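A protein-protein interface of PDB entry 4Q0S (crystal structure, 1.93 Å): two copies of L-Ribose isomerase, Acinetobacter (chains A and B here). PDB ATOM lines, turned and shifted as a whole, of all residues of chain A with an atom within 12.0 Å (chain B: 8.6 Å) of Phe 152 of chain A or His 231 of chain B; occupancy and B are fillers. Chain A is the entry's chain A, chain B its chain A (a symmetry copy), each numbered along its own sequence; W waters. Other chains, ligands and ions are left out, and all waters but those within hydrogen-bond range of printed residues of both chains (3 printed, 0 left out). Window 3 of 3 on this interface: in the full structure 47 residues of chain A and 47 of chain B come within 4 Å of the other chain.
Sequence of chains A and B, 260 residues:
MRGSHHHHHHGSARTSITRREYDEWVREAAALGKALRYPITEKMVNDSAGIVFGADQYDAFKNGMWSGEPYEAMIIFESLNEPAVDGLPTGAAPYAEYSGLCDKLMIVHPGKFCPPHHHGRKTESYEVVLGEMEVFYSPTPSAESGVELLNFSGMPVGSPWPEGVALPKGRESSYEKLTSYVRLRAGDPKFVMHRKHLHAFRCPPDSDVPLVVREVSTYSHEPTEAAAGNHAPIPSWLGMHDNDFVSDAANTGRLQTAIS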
ATOM      1  N   THR A 123      14.984 -23.304  -5.742  1.00  0.00           N
ATOM      2  CA  THR A 123      14.313 -22.838  -6.946  1.00  0.00           C
ATOM      3  C   THR A 123      14.036 -21.346  -6.692  1.00  0.00           C
ATOM      4  O   THR A 123      13.525 -20.973  -5.627  1.00  0.00           O
ATOM      5  CB  THR A 123      12.977 -23.578  -7.173  1.00  0.00           C
ATOM      6  OG1 THR A 123      13.238 -24.907  -7.643  1.00  0.00           O
ATOM      7  CG2 THR A 123      12.120 -22.829  -8.191  1.00  0.00           C
ATOM      8  N   PRO A 139      19.058 -24.100 -20.162  1.00  0.00           N
ATOM      9  CA  PRO A 139      17.679 -24.592 -20.212  1.00  0.00           C
ATOM     10  C   PRO A 139      17.513 -26.037 -19.730  1.00  0.00           C
ATOM     11  O   PRO A 139      16.390 -26.489 -19.478  1.00  0.00           O
ATOM     12  CB  PRO A 139      17.303 -24.401 -21.677  1.00  0.00           C
ATOM     13  CG  PRO A 139      18.599 -24.622 -22.374  1.00  0.00           C
ATOM     14  CD  PRO A 139      19.581 -23.864 -21.518  1.00  0.00           C
ATOM     15  N   THR A 140      18.621 -26.764 -19.603  1.00  0.00           N
ATOM     16  CA  THR A 140      18.557 -28.137 -19.108  1.00  0.00           C
ATOM     17  C   THR A 140      19.166 -28.187 -17.718  1.00  0.00           C
ATOM     18  O   THR A 140      20.142 -27.496 -17.431  1.00  0.00           O
ATOM     19  CB  THR A 140      19.315 -29.144 -20.016  1.00  0.00           C
ATOM     20  OG1 THR A 140      20.617 -28.639 -20.320  1.00  0.00           O
ATOM     21  CG2 THR A 140      18.555 -29.387 -21.292  1.00  0.00           C
ATOM     22  N   PRO A 141      18.586 -29.002 -16.828  1.00  0.00           N
ATOM     23  CA  PRO A 141      19.121 -29.101 -15.471  1.00  0.00           C
ATOM     24  C   PRO A 141      20.403 -29.913 -15.464  1.00  0.00           C
ATOM     25  O   PRO A 141      20.737 -30.561 -16.456  1.00  0.00           O
ATOM     26  CB  PRO A 141      17.997 -29.798 -14.714  1.00  0.00           C
ATOM     27  CG  PRO A 141      17.442 -30.718 -15.752  1.00  0.00           C
ATOM     28  CD  PRO A 141      17.374 -29.826 -16.976  1.00  0.00           C
ATOM     29  N   GLU A 148      16.528 -40.241  -9.562  1.00  0.00           N
ATOM     30  CA  GLU A 148      15.449 -39.865 -10.466  1.00  0.00           C
ATOM     31  C   GLU A 148      14.870 -38.543  -9.978  1.00  0.00           C
ATOM     32  O   GLU A 148      14.692 -38.341  -8.778  1.00  0.00           O
ATOM     33  CB  GLU A 148      14.361 -40.941 -10.452  1.00  0.00           C
ATOM     34  CG  GLU A 148      13.862 -41.363 -11.828  1.00  0.00           C
ATOM     35  CD  GLU A 148      13.171 -40.241 -12.583  1.00  0.00           C
ATOM     36  OE1 GLU A 148      13.830 -39.219 -12.874  1.00  0.00           O
ATOM     37  OE2 GLU A 148      11.967 -40.384 -12.888  1.00  0.00           O
ATOM     38  N   LEU A 149      14.582 -37.644 -10.911  1.00  0.00           N
ATOM     39  CA  LEU A 149      14.030 -36.340 -10.561  1.00  0.00           C
ATOM     40  C   LEU A 149      12.660 -36.104 -11.188  1.00  0.00           C
ATOM     41  O   LEU A 149      12.384 -36.556 -12.301  1.00  0.00           O
ATOM     42  CB  LEU A 149      14.990 -35.235 -11.003  1.00  0.00           C
ATOM     43  CG  LEU A 149      16.424 -35.345 -10.483  1.00  0.00           C
ATOM     44  CD1 LEU A 149      17.268 -34.252 -11.099  1.00  0.00           C
ATOM     45  CD2 LEU A 149      16.442 -35.247  -8.968  1.00  0.00           C
ATOM     46  N   LEU A 150      11.804 -35.393 -10.466  1.00  0.00           N
ATOM     47  CA  LEU A 150      10.473 -35.081 -10.961  1.00  0.00           C
ATOM     48  C   LEU A 150      10.587 -33.988 -12.021  1.00  0.00           C
ATOM     49  O   LEU A 150      11.593 -33.283 -12.089  1.00  0.00           O
ATOM     50  CB  LEU A 150       9.585 -34.605  -9.814  1.00  0.00           C
ATOM     51  CG  LEU A 150       9.396 -35.594  -8.662  1.00  0.00           C
ATOM     52  CD1 LEU A 150       8.483 -34.991  -7.608  1.00  0.00           C
ATOM     53  CD2 LEU A 150       8.807 -36.891  -9.200  1.00  0.00           C
ATOM     54  N   ASN A 151       9.559 -33.865 -12.852  1.00  0.00           N
ATOM     55  CA  ASN A 151       9.527 -32.867 -13.913  1.00  0.00           C
ATOM     56  C   ASN A 151       8.098 -32.397 -14.127  1.00  0.00           C
ATOM     57  O   ASN A 151       7.154 -33.171 -13.973  1.00  0.00           O
ATOM     58  CB  ASN A 151      10.058 -33.454 -15.223  1.00  0.00           C
ATOM     59  CG  ASN A 151      11.509 -33.880 -15.125  1.00  0.00           C
ATOM     60  OD1 ASN A 151      12.394 -33.065 -14.850  1.00  0.00           O
ATOM     61  ND2 ASN A 151      11.764 -35.167 -15.352  1.00  0.00           N
ATOM     62  N   PHE A 152       7.937 -31.119 -14.455  1.00  0.00           N
ATOM     63  CA  PHE A 152       6.613 -30.568 -14.699  1.00  0.00           C
ATOM     64  C   PHE A 152       6.602 -29.501 -15.792  1.00  0.00           C
ATOM     65  O   PHE A 152       5.960 -29.665 -16.827  1.00  0.00           O
ATOM     66  CB  PHE A 152       6.048 -29.988 -13.402  1.00  0.00           C
ATOM     67  CG  PHE A 152       4.737 -29.279 -13.576  1.00  0.00           C
ATOM     68  CD1 PHE A 152       3.653 -29.928 -14.166  1.00  0.00           C
ATOM     69  CD2 PHE A 152       4.583 -27.961 -13.152  1.00  0.00           C
ATOM     70  CE1 PHE A 152       2.434 -29.277 -14.330  1.00  0.00           C
ATOM     71  CE2 PHE A 152       3.369 -27.298 -13.310  1.00  0.00           C
ATOM     72  CZ  PHE A 152       2.289 -27.957 -13.902  1.00  0.00           C
ATOM     73  N   SER A 153       7.308 -28.400 -15.562  1.00  0.00           N
ATOM     74  CA  SER A 153       7.328 -27.322 -16.549  1.00  0.00           C
ATOM     75  C   SER A 153       8.679 -27.132 -17.207  1.00  0.00           C
ATOM     76  O   SER A 153       8.761 -26.588 -18.310  1.00  0.00           O
ATOM     77  CB  SER A 153       6.897 -26.008 -15.897  1.00  0.00           C
ATOM     78  OG  SER A 153       7.744 -25.692 -14.808  1.00  0.00           O
ATOM     79  N   GLY A 154       9.735 -27.582 -16.543  1.00  0.00           N
ATOM     80  CA  GLY A 154      11.066 -27.409 -17.095  1.00  0.00           C
ATOM     81  C   GLY A 154      11.334 -25.927 -17.290  1.00  0.00           C
ATOM     82  O   GLY A 154      10.567 -25.096 -16.804  1.00  0.00           O
ATOM     83  N   MET A 155      12.411 -25.592 -17.994  1.00  0.00           N
ATOM     84  CA  MET A 155      12.757 -24.199 -18.249  1.00  0.00           C
ATOM     85  C   MET A 155      12.590 -23.864 -19.723  1.00  0.00           C
ATOM     86  O   MET A 155      12.878 -24.689 -20.594  1.00  0.00           O
ATOM     87  CB  MET A 155      14.214 -23.916 -17.849  1.00  0.00           C
ATOM     88  CG  MET A 155      14.479 -23.875 -16.354  1.00  0.00           C
ATOM     89  SD  MET A 155      13.729 -22.433 -15.551  1.00  0.00           S
ATOM     90  CE  MET A 155      14.571 -21.116 -16.390  1.00  0.00           C
ATOM     91  N   PRO A 156      12.119 -22.646 -20.025  1.00  0.00           N
ATOM     92  CA  PRO A 156      11.934 -22.227 -21.421  1.00  0.00           C
ATOM     93  C   PRO A 156      13.296 -22.060 -22.094  1.00  0.00           C
ATOM     94  O   PRO A 156      14.285 -21.725 -21.440  1.00  0.00           O
ATOM     95  CB  PRO A 156      11.180 -20.903 -21.288  1.00  0.00           C
ATOM     96  CG  PRO A 156      11.670 -20.370 -19.960  1.00  0.00           C
ATOM     97  CD  PRO A 156      11.650 -21.606 -19.092  1.00  0.00           C
ATOM     98  N   VAL A 192      10.700 -17.824 -13.242  1.00  0.00           N
ATOM     99  CA  VAL A 192      11.156 -18.958 -12.443  1.00  0.00           C
ATOM    100  C   VAL A 192      12.461 -19.605 -12.907  1.00  0.00           C
ATOM    101  O   VAL A 192      12.624 -19.956 -14.074  1.00  0.00           O
ATOM    102  CB  VAL A 192      10.065 -20.066 -12.386  1.00  0.00           C
ATOM    103  CG1 VAL A 192      10.583 -21.291 -11.637  1.00  0.00           C
ATOM    104  CG2 VAL A 192       8.821 -19.521 -11.704  1.00  0.00           C
ATOM    105  N   MET A 193      13.393 -19.755 -11.976  1.00  0.00           N
ATOM    106  CA  MET A 193      14.666 -20.403 -12.266  1.00  0.00           C
ATOM    107  C   MET A 193      14.639 -21.675 -11.425  1.00  0.00           C
ATOM    108  O   MET A 193      14.898 -21.636 -10.220  1.00  0.00           O
ATOM    109  CB  MET A 193      15.840 -19.517 -11.842  1.00  0.00           C
ATOM    110  CG  MET A 193      17.222 -20.119 -12.122  1.00  0.00           C
ATOM    111  SD  MET A 193      17.491 -20.501 -13.882  1.00  0.00           S
ATOM    112  CE  MET A 193      17.331 -18.846 -14.638  1.00  0.00           C
ATOM    113  N   HIS A 194      14.299 -22.801 -12.051  1.00  0.00           N
ATOM    114  CA  HIS A 194      14.231 -24.060 -11.318  1.00  0.00           C
ATOM    115  C   HIS A 194      15.577 -24.472 -10.755  1.00  0.00           C
ATOM    116  O   HIS A 194      16.634 -24.130 -11.299  1.00  0.00           O
ATOM    117  CB  HIS A 194      13.708 -25.192 -12.210  1.00  0.00           C
ATOM    118  CG  HIS A 194      12.247 -25.096 -12.519  1.00  0.00           C
ATOM    119  ND1 HIS A 194      11.281 -25.023 -11.538  1.00  0.00           N
ATOM    120  CD2 HIS A 194      11.585 -25.085 -13.700  1.00  0.00           C
ATOM    121  CE1 HIS A 194      10.086 -24.973 -12.101  1.00  0.00           C
ATOM    122  NE2 HIS A 194      10.243 -25.009 -13.412  1.00  0.00           N
ATOM    123  N   ARG A 195      15.527 -25.208  -9.652  1.00  0.00           N
ATOM    124  CA  ARG A 195      16.728 -25.713  -9.023  1.00  0.00           C
ATOM    125  C   ARG A 195      17.445 -26.596 -10.046  1.00  0.00           C
ATOM    126  O   ARG A 195      16.824 -27.100 -10.979  1.00  0.00           O
ATOM    127  CB  ARG A 195      16.357 -26.539  -7.791  1.00  0.00           C
ATOM    128  CG  ARG A 195      15.374 -27.666  -8.089  1.00  0.00           C
ATOM    129  CD  ARG A 195      15.145 -28.541  -6.872  1.00  0.00           C
ATOM    130  NE  ARG A 195      14.297 -27.904  -5.869  1.00  0.00           N
ATOM    131  CZ  ARG A 195      12.974 -27.811  -5.959  1.00  0.00           C
ATOM    132  NH1 ARG A 195      12.344 -28.317  -7.008  1.00  0.00           N
ATOM    133  NH2 ARG A 195      12.282 -27.221  -4.993  1.00  0.00           N
ATOM    134  N   LYS A 196      18.751 -26.761  -9.853  1.00  0.00           N
ATOM    135  CA  LYS A 196      19.619 -27.571 -10.703  1.00  0.00           C
ATOM    136  C   LYS A 196      19.915 -26.957 -12.065  1.00  0.00           C
ATOM    137  O   LYS A 196      20.510 -27.600 -12.928  1.00  0.00           O
ATOM    138  CB  LYS A 196      19.052 -28.990 -10.855  1.00  0.00           C
ATOM    139  CG  LYS A 196      19.098 -29.792  -9.548  1.00  0.00           C
ATOM    140  CD  LYS A 196      18.552 -31.199  -9.726  1.00  0.00           C
ATOM    141  CE  LYS A 196      18.796 -32.052  -8.485  1.00  0.00           C
ATOM    142  NZ  LYS A 196      18.123 -31.482  -7.293  1.00  0.00           N
ATOM    143  N   HIS A 197      19.521 -25.701 -12.246  1.00  0.00           N
ATOM    144  CA  HIS A 197      19.781 -25.002 -13.498  1.00  0.00           C
ATOM    145  C   HIS A 197      20.860 -23.957 -13.323  1.00  0.00           C
ATOM    146  O   HIS A 197      20.797 -23.145 -12.403  1.00  0.00           O
ATOM    147  CB  HIS A 197      18.511 -24.321 -14.005  1.00  0.00           C
ATOM    148  CG  HIS A 197      17.570 -25.253 -14.690  1.00  0.00           C
ATOM    149  ND1 HIS A 197      17.633 -25.507 -16.043  1.00  0.00           N
ATOM    150  CD2 HIS A 197      16.583 -26.039 -14.202  1.00  0.00           C
ATOM    151  CE1 HIS A 197      16.726 -26.414 -16.358  1.00  0.00           C
ATOM    152  NE2 HIS A 197      16.077 -26.754 -15.259  1.00  0.00           N
ATOM    153  N   ASN B  81       2.488 -18.819  -8.542  1.00  0.00           N
ATOM    154  CA  ASN B  81       1.999 -19.973  -7.805  1.00  0.00           C
ATOM    155  C   ASN B  81       2.729 -21.117  -8.488  1.00  0.00           C
ATOM    156  O   ASN B  81       2.169 -21.868  -9.286  1.00  0.00           O
ATOM    157  CB  ASN B  81       0.479 -20.113  -7.920  1.00  0.00           C
ATOM    158  CG  ASN B  81      -0.098 -21.012  -6.842  1.00  0.00           C
ATOM    159  OD1 ASN B  81       0.451 -21.110  -5.739  1.00  0.00           O
ATOM    160  ND2 ASN B  81      -1.213 -21.659  -7.145  1.00  0.00           N
ATOM    161  N   GLU B  82       4.016 -21.189  -8.172  1.00  0.00           N
ATOM    162  CA  GLU B  82       4.940 -22.160  -8.721  1.00  0.00           C
ATOM    163  C   GLU B  82       5.017 -23.429  -7.880  1.00  0.00           C
ATOM    164  O   GLU B  82       5.348 -23.384  -6.696  1.00  0.00           O
ATOM    165  CB  GLU B  82       6.321 -21.507  -8.829  1.00  0.00           C
ATOM    166  CG  GLU B  82       7.472 -22.458  -9.086  1.00  0.00           C
ATOM    167  CD  GLU B  82       7.279 -23.287 -10.336  1.00  0.00           C
ATOM    168  OE1 GLU B  82       6.793 -22.737 -11.349  1.00  0.00           O
ATOM    169  OE2 GLU B  82       7.626 -24.487 -10.305  1.00  0.00           O
ATOM    170  N   PRO B  83       4.715 -24.584  -8.493  1.00  0.00           N
ATOM    171  CA  PRO B  83       4.758 -25.862  -7.778  1.00  0.00           C
ATOM    172  C   PRO B  83       6.146 -26.170  -7.226  1.00  0.00           C
ATOM    173  O   PRO B  83       6.273 -26.737  -6.144  1.00  0.00           O
ATOM    174  CB  PRO B  83       4.328 -26.873  -8.844  1.00  0.00           C
ATOM    175  CG  PRO B  83       3.395 -26.074  -9.708  1.00  0.00           C
ATOM    176  CD  PRO B  83       4.156 -24.758  -9.845  1.00  0.00           C
ATOM    177  N   ALA B  84       7.178 -25.776  -7.970  1.00  0.00           N
ATOM    178  CA  ALA B  84       8.566 -26.032  -7.580  1.00  0.00           C
ATOM    179  C   ALA B  84       8.810 -27.547  -7.518  1.00  0.00           C
ATOM    180  O   ALA B  84       9.552 -28.047  -6.669  1.00  0.00           O
ATOM    181  CB  ALA B  84       8.870 -25.388  -6.233  1.00  0.00           C
ATOM    182  N   VAL B  85       8.175 -28.266  -8.435  1.00  0.00           N
ATOM    183  CA  VAL B  85       8.295 -29.718  -8.506  1.00  0.00           C
ATOM    184  C   VAL B  85       9.495 -30.151  -9.338  1.00  0.00           C
ATOM    185  O   VAL B  85      10.065 -31.214  -9.095  1.00  0.00           O
ATOM    186  CB  VAL B  85       7.003 -30.345  -9.092  1.00  0.00           C
ATOM    187  CG1 VAL B  85       7.288 -31.722  -9.676  1.00  0.00           C
ATOM    188  CG2 VAL B  85       5.950 -30.447  -7.994  1.00  0.00           C
ATOM    189  N   ASP B  86       9.879 -29.326 -10.310  1.00  0.00           N
ATOM    190  CA  ASP B  86      11.016 -29.637 -11.172  1.00  0.00           C
ATOM    191  C   ASP B  86      12.331 -29.725 -10.421  1.00  0.00           C
ATOM    192  O   ASP B  86      12.672 -28.831  -9.644  1.00  0.00           O
ATOM    193  CB  ASP B  86      11.153 -28.593 -12.284  1.00  0.00           C
ATOM    194  CG  ASP B  86      10.026 -28.663 -13.283  1.00  0.00           C
ATOM    195  OD1 ASP B  86       8.918 -28.169 -12.982  1.00  0.00           O
ATOM    196  OD2 ASP B  86      10.244 -29.230 -14.372  1.00  0.00           O
ATOM    197  N   GLY B  87      13.073 -30.804 -10.662  1.00  0.00           N
ATOM    198  CA  GLY B  87      14.356 -30.977 -10.008  1.00  0.00           C
ATOM    199  C   GLY B  87      14.294 -31.687  -8.671  1.00  0.00           C
ATOM    200  O   GLY B  87      15.328 -31.921  -8.043  1.00  0.00           O
ATOM    201  N   LEU B  88      13.092 -32.030  -8.226  1.00  0.00           N
ATOM    202  CA  LEU B  88      12.930 -32.722  -6.954  1.00  0.00           C
ATOM    203  C   LEU B  88      13.177 -34.217  -7.068  1.00  0.00           C
ATOM    204  O   LEU B  88      12.876 -34.829  -8.091  1.00  0.00           O
ATOM    205  CB  LEU B  88      11.512 -32.541  -6.415  1.00  0.00           C
ATOM    206  CG  LEU B  88      11.091 -31.224  -5.772  1.00  0.00           C
ATOM    207  CD1 LEU B  88       9.623 -31.314  -5.383  1.00  0.00           C
ATOM    208  CD2 LEU B  88      11.947 -30.954  -4.550  1.00  0.00           C
ATOM    209  N   TYR B 219       3.141 -23.127  -2.133  1.00  0.00           N
ATOM    210  CA  TYR B 219       2.093 -23.317  -3.134  1.00  0.00           C
ATOM    211  C   TYR B 219       0.656 -23.201  -2.632  1.00  0.00           C
ATOM    212  O   TYR B 219       0.310 -23.713  -1.569  1.00  0.00           O
ATOM    213  CB  TYR B 219       2.270 -24.669  -3.822  1.00  0.00           C
ATOM    214  CG  TYR B 219       1.443 -24.829  -5.075  1.00  0.00           C
ATOM    215  CD1 TYR B 219       1.846 -24.252  -6.278  1.00  0.00           C
ATOM    216  CD2 TYR B 219       0.259 -25.569  -5.063  1.00  0.00           C
ATOM    217  CE1 TYR B 219       1.092 -24.409  -7.441  1.00  0.00           C
ATOM    218  CE2 TYR B 219      -0.506 -25.737  -6.223  1.00  0.00           C
ATOM    219  CZ  TYR B 219      -0.080 -25.155  -7.406  1.00  0.00           C
ATOM    220  OH  TYR B 219      -0.815 -25.331  -8.555  1.00  0.00           O
ATOM    221  N   ALA B 227      -8.505 -20.891 -11.720  1.00  0.00           N
ATOM    222  CA  ALA B 227      -7.567 -22.006 -11.669  1.00  0.00           C
ATOM    223  C   ALA B 227      -8.289 -23.347 -11.801  1.00  0.00           C
ATOM    224  O   ALA B 227      -7.990 -24.298 -11.076  1.00  0.00           O
ATOM    225  CB  ALA B 227      -6.777 -21.961 -10.362  1.00  0.00           C
ATOM    226  N   ALA B 228      -9.238 -23.417 -12.730  1.00  0.00           N
ATOM    227  CA  ALA B 228      -9.999 -24.642 -12.953  1.00  0.00           C
ATOM    228  C   ALA B 228      -9.825 -25.144 -14.383  1.00  0.00           C
ATOM    229  O   ALA B 228     -10.646 -24.856 -15.255  1.00  0.00           O
ATOM    230  CB  ALA B 228     -11.478 -24.399 -12.658  1.00  0.00           C
ATOM    231  N   GLY B 229      -8.752 -25.896 -14.620  1.00  0.00           N
ATOM    232  CA  GLY B 229      -8.500 -26.427 -15.949  1.00  0.00           C
ATOM    233  C   GLY B 229      -7.027 -26.586 -16.286  1.00  0.00           C
ATOM    234  O   GLY B 229      -6.683 -27.031 -17.382  1.00  0.00           O
ATOM    235  N   ASN B 230      -6.157 -26.228 -15.344  1.00  0.00           N
ATOM    236  CA  ASN B 230      -4.713 -26.329 -15.547  1.00  0.00           C
ATOM    237  C   ASN B 230      -4.225 -27.774 -15.437  1.00  0.00           C
ATOM    238  O   ASN B 230      -5.025 -28.702 -15.308  1.00  0.00           O
ATOM    239  CB  ASN B 230      -3.978 -25.463 -14.518  1.00  0.00           C
ATOM    240  CG  ASN B 230      -4.395 -24.006 -14.574  1.00  0.00           C
ATOM    241  OD1 ASN B 230      -4.256 -23.347 -15.606  1.00  0.00           O
ATOM    242  ND2 ASN B 230      -4.908 -23.492 -13.461  1.00  0.00           N
ATOM    243  N   HIS B 231      -2.908 -27.957 -15.492  1.00  0.00           N
ATOM    244  CA  HIS B 231      -2.306 -29.283 -15.389  1.00  0.00           C
ATOM    245  C   HIS B 231      -1.765 -29.487 -13.974  1.00  0.00           C
ATOM    246  O   HIS B 231      -1.259 -28.549 -13.356  1.00  0.00           O
ATOM    247  CB  HIS B 231      -1.164 -29.428 -16.403  1.00  0.00           C
ATOM    248  CG  HIS B 231      -0.537 -30.791 -16.427  1.00  0.00           C
ATOM    249  ND1 HIS B 231       0.610 -31.068 -17.141  1.00  0.00           N
ATOM    250  CD2 HIS B 231      -0.897 -31.953 -15.833  1.00  0.00           C
ATOM    251  CE1 HIS B 231       0.930 -32.340 -16.982  1.00  0.00           C
ATOM    252  NE2 HIS B 231       0.032 -32.899 -16.193  1.00  0.00           N
ATOM    253  N   ALA B 232      -1.876 -30.712 -13.465  1.00  0.00           N
ATOM    254  CA  ALA B 232      -1.396 -31.037 -12.126  1.00  0.00           C
ATOM    255  C   ALA B 232       0.034 -31.566 -12.175  1.00  0.00           C
ATOM    256  O   ALA B 232       0.314 -32.566 -12.839  1.00  0.00           O
ATOM    257  CB  ALA B 232      -2.311 -32.068 -11.476  1.00  0.00           C
ATOM    258  N   PRO B 233       0.960 -30.898 -11.469  1.00  0.00           N
ATOM    259  CA  PRO B 233       2.368 -31.309 -11.434  1.00  0.00           C
ATOM    260  C   PRO B 233       2.551 -32.692 -10.821  1.00  0.00           C
ATOM    261  O   PRO B 233       3.459 -33.433 -11.191  1.00  0.00           O
ATOM    262  CB  PRO B 233       3.027 -30.206 -10.610  1.00  0.00           C
ATOM    263  CG  PRO B 233       1.927 -29.771  -9.695  1.00  0.00           C
ATOM    264  CD  PRO B 233       0.738 -29.719 -10.615  1.00  0.00           C
ATOM    265  N   ILE B 234       1.683 -33.021  -9.872  1.00  0.00           N
ATOM    266  CA  ILE B 234       1.709 -34.318  -9.208  1.00  0.00           C
ATOM    267  C   ILE B 234       0.263 -34.792  -9.126  1.00  0.00           C
ATOM    268  O   ILE B 234      -0.637 -34.009  -8.819  1.00  0.00           O
ATOM    269  CB  ILE B 234       2.327 -34.220  -7.790  1.00  0.00           C
ATOM    270  CG1 ILE B 234       3.826 -33.939  -7.904  1.00  0.00           C
ATOM    271  CG2 ILE B 234       2.094 -35.513  -7.017  1.00  0.00           C
ATOM    272  CD1 ILE B 234       4.539 -33.829  -6.577  1.00  0.00           C
ATOM    273  N   PRO B 235       0.018 -36.080  -9.422  1.00  0.00           N
ATOM    274  CA  PRO B 235      -1.319 -36.680  -9.393  1.00  0.00           C
ATOM    275  C   PRO B 235      -2.220 -36.219  -8.250  1.00  0.00           C
ATOM    276  O   PRO B 235      -3.268 -35.619  -8.486  1.00  0.00           O
ATOM    277  CB  PRO B 235      -1.015 -38.171  -9.339  1.00  0.00           C
ATOM    278  CG  PRO B 235       0.183 -38.266 -10.230  1.00  0.00           C
ATOM    279  CD  PRO B 235       1.033 -37.095  -9.769  1.00  0.00           C
ATOM    280  N   TRP B 237      -2.175 -33.759  -6.275  1.00  0.00           N
ATOM    281  CA  TRP B 237      -2.500 -32.334  -6.291  1.00  0.00           C
ATOM    282  C   TRP B 237      -3.834 -32.027  -6.965  1.00  0.00           C
ATOM    283  O   TRP B 237      -4.469 -31.017  -6.664  1.00  0.00           O
ATOM    284  CB  TRP B 237      -1.393 -31.556  -7.002  1.00  0.00           C
ATOM    285  CG  TRP B 237      -0.105 -31.483  -6.242  1.00  0.00           C
ATOM    286  CD1 TRP B 237       0.464 -32.470  -5.487  1.00  0.00           C
ATOM    287  CD2 TRP B 237       0.813 -30.384  -6.222  1.00  0.00           C
ATOM    288  NE1 TRP B 237       1.683 -32.056  -5.003  1.00  0.00           N
ATOM    289  CE2 TRP B 237       1.922 -30.779  -5.440  1.00  0.00           C
ATOM    290  CE3 TRP B 237       0.808 -29.104  -6.794  1.00  0.00           C
ATOM    291  CZ2 TRP B 237       3.019 -29.938  -5.216  1.00  0.00           C
ATOM    292  CZ3 TRP B 237       1.899 -28.268  -6.572  1.00  0.00           C
ATOM    293  CH2 TRP B 237       2.990 -28.691  -5.789  1.00  0.00           C
ATOM    294  N   LEU B 238      -4.252 -32.899  -7.878  1.00  0.00           N
ATOM    295  CA  LEU B 238      -5.504 -32.712  -8.606  1.00  0.00           C
ATOM    296  C   LEU B 238      -6.724 -32.636  -7.690  1.00  0.00           C
ATOM    297  O   LEU B 238      -7.008 -33.570  -6.938  1.00  0.00           O
ATOM    298  CB  LEU B 238      -5.692 -33.846  -9.617  1.00  0.00           C
ATOM    299  CG  LEU B 238      -6.954 -33.803 -10.482  1.00  0.00           C
ATOM    300  CD1 LEU B 238      -7.005 -32.508 -11.280  1.00  0.00           C
ATOM    301  CD2 LEU B 238      -6.957 -35.005 -11.412  1.00  0.00           C
HETATM  302  O   HOH W   1      11.355 -26.124  -9.192  1.00  0.00           O
HETATM  303  O   HOH W   2       9.808 -28.281  -3.478  1.00  0.00           O
HETATM  304  O   HOH W   3      15.173 -28.942 -12.524  1.00  0.00           O
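Water W2 lies within hydrogen-bond range of NH2 of Arg 195 of chain A and O of Ala 84 of chain B.
No position is printed for both chains. Of the 22 pairs that touch across the chains among the printed residues, none has its exchanged pair printed and touching as well.
The side-chain sulfur (SD) of Met 155 of chain A is in hydrogen-bond range of the backbone NH (N) of His 194 of chain A (3.6 Å). N of Arg 195 of chain A lies within hydrogen-bond range of OG1 of Thr 123 of chain A (3.1 Å).
The guanidinium group (NH1) of Arg 195 of chain A sits at hydrogen-bond distance from the backbone carbonyl oxygen (O) of Ala 84 of chain B (2.8 Å). The guanidinium group of Arg 195 of chain A sits at hydrogen-bond distance from the backbone carbonyl oxygen of Asp 86 of chain B (2.7 Å). The side-chain carboxylate of Asp 86 of chain B is in hydrogen-bond range of the backbone NH of Ser 153 of chain A (3.0 Å). N of Phe 152 of chain A lies within hydrogen-bond range of OD2 of Asp 86 of chain B (3.0 Å). O of Leu 150 of chain A sits at hydrogen-bond distance from N of Gly 87 of chain B (3.2 Å). The backbone carbonyl oxygen (O) of Leu 88 of chain B sits at hydrogen-bond distance from the backbone NH (N) of Leu 150 of chain A. The side-chain amino group (NZ) of Lys 196 of chain A is in hydrogen-bond range of the backbone carbonyl oxygen (O) of Gly 87 of chain B (2.9 Å). The backbone NH of Gly 154 of chain A lies within hydrogen-bond range of the side-chain carboxylate of Asp 86 of chain B (2.8 Å). A ring nitrogen (NE2) of His 194 of chain A sits at hydrogen-bond distance from the side-chain carboxylate of Asp 86 of chain B, at 3.5 Å.
Along chain B the printed residues that touch a printed residue of chain A span positions 82 to 233. Of the 19 printed residues of chain A, 10 touch a printed residue of chain B. Among the printed residues, 22 pairs touch across the chains. Among the printed residues, no Asp or Glu carboxylate lies within 4 Å of a Lys or Arg side-chain nitrogen of the other chain.
Phe 152 of chain A touches five residues of chain B. Of chain A, only Phe 152 comes within 4 Å of His 231 of chain B. Pro 83 of chain B touches one residue of chain A. No residue of chain A comes within 4 Å of Gly 229 of chain B. Of the printed residues of chain B, Val 192 of chain A touches Glu 82. Of the printed residues of chain A, Ala 84 of chain B touches Arg 195. Printed residues of chain B within 4 Å of Arg 195 of chain A: Ala 84, Asp 86, Gly 87 and Leu 88. The nearest residue of chain A that does not touch His 231 of chain B is Asn 151 of chain A (7.0 Å). The nearest printed residue of chain B that does not touch His 194 of chain A is Ala 84 of chain B (4.9 Å).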
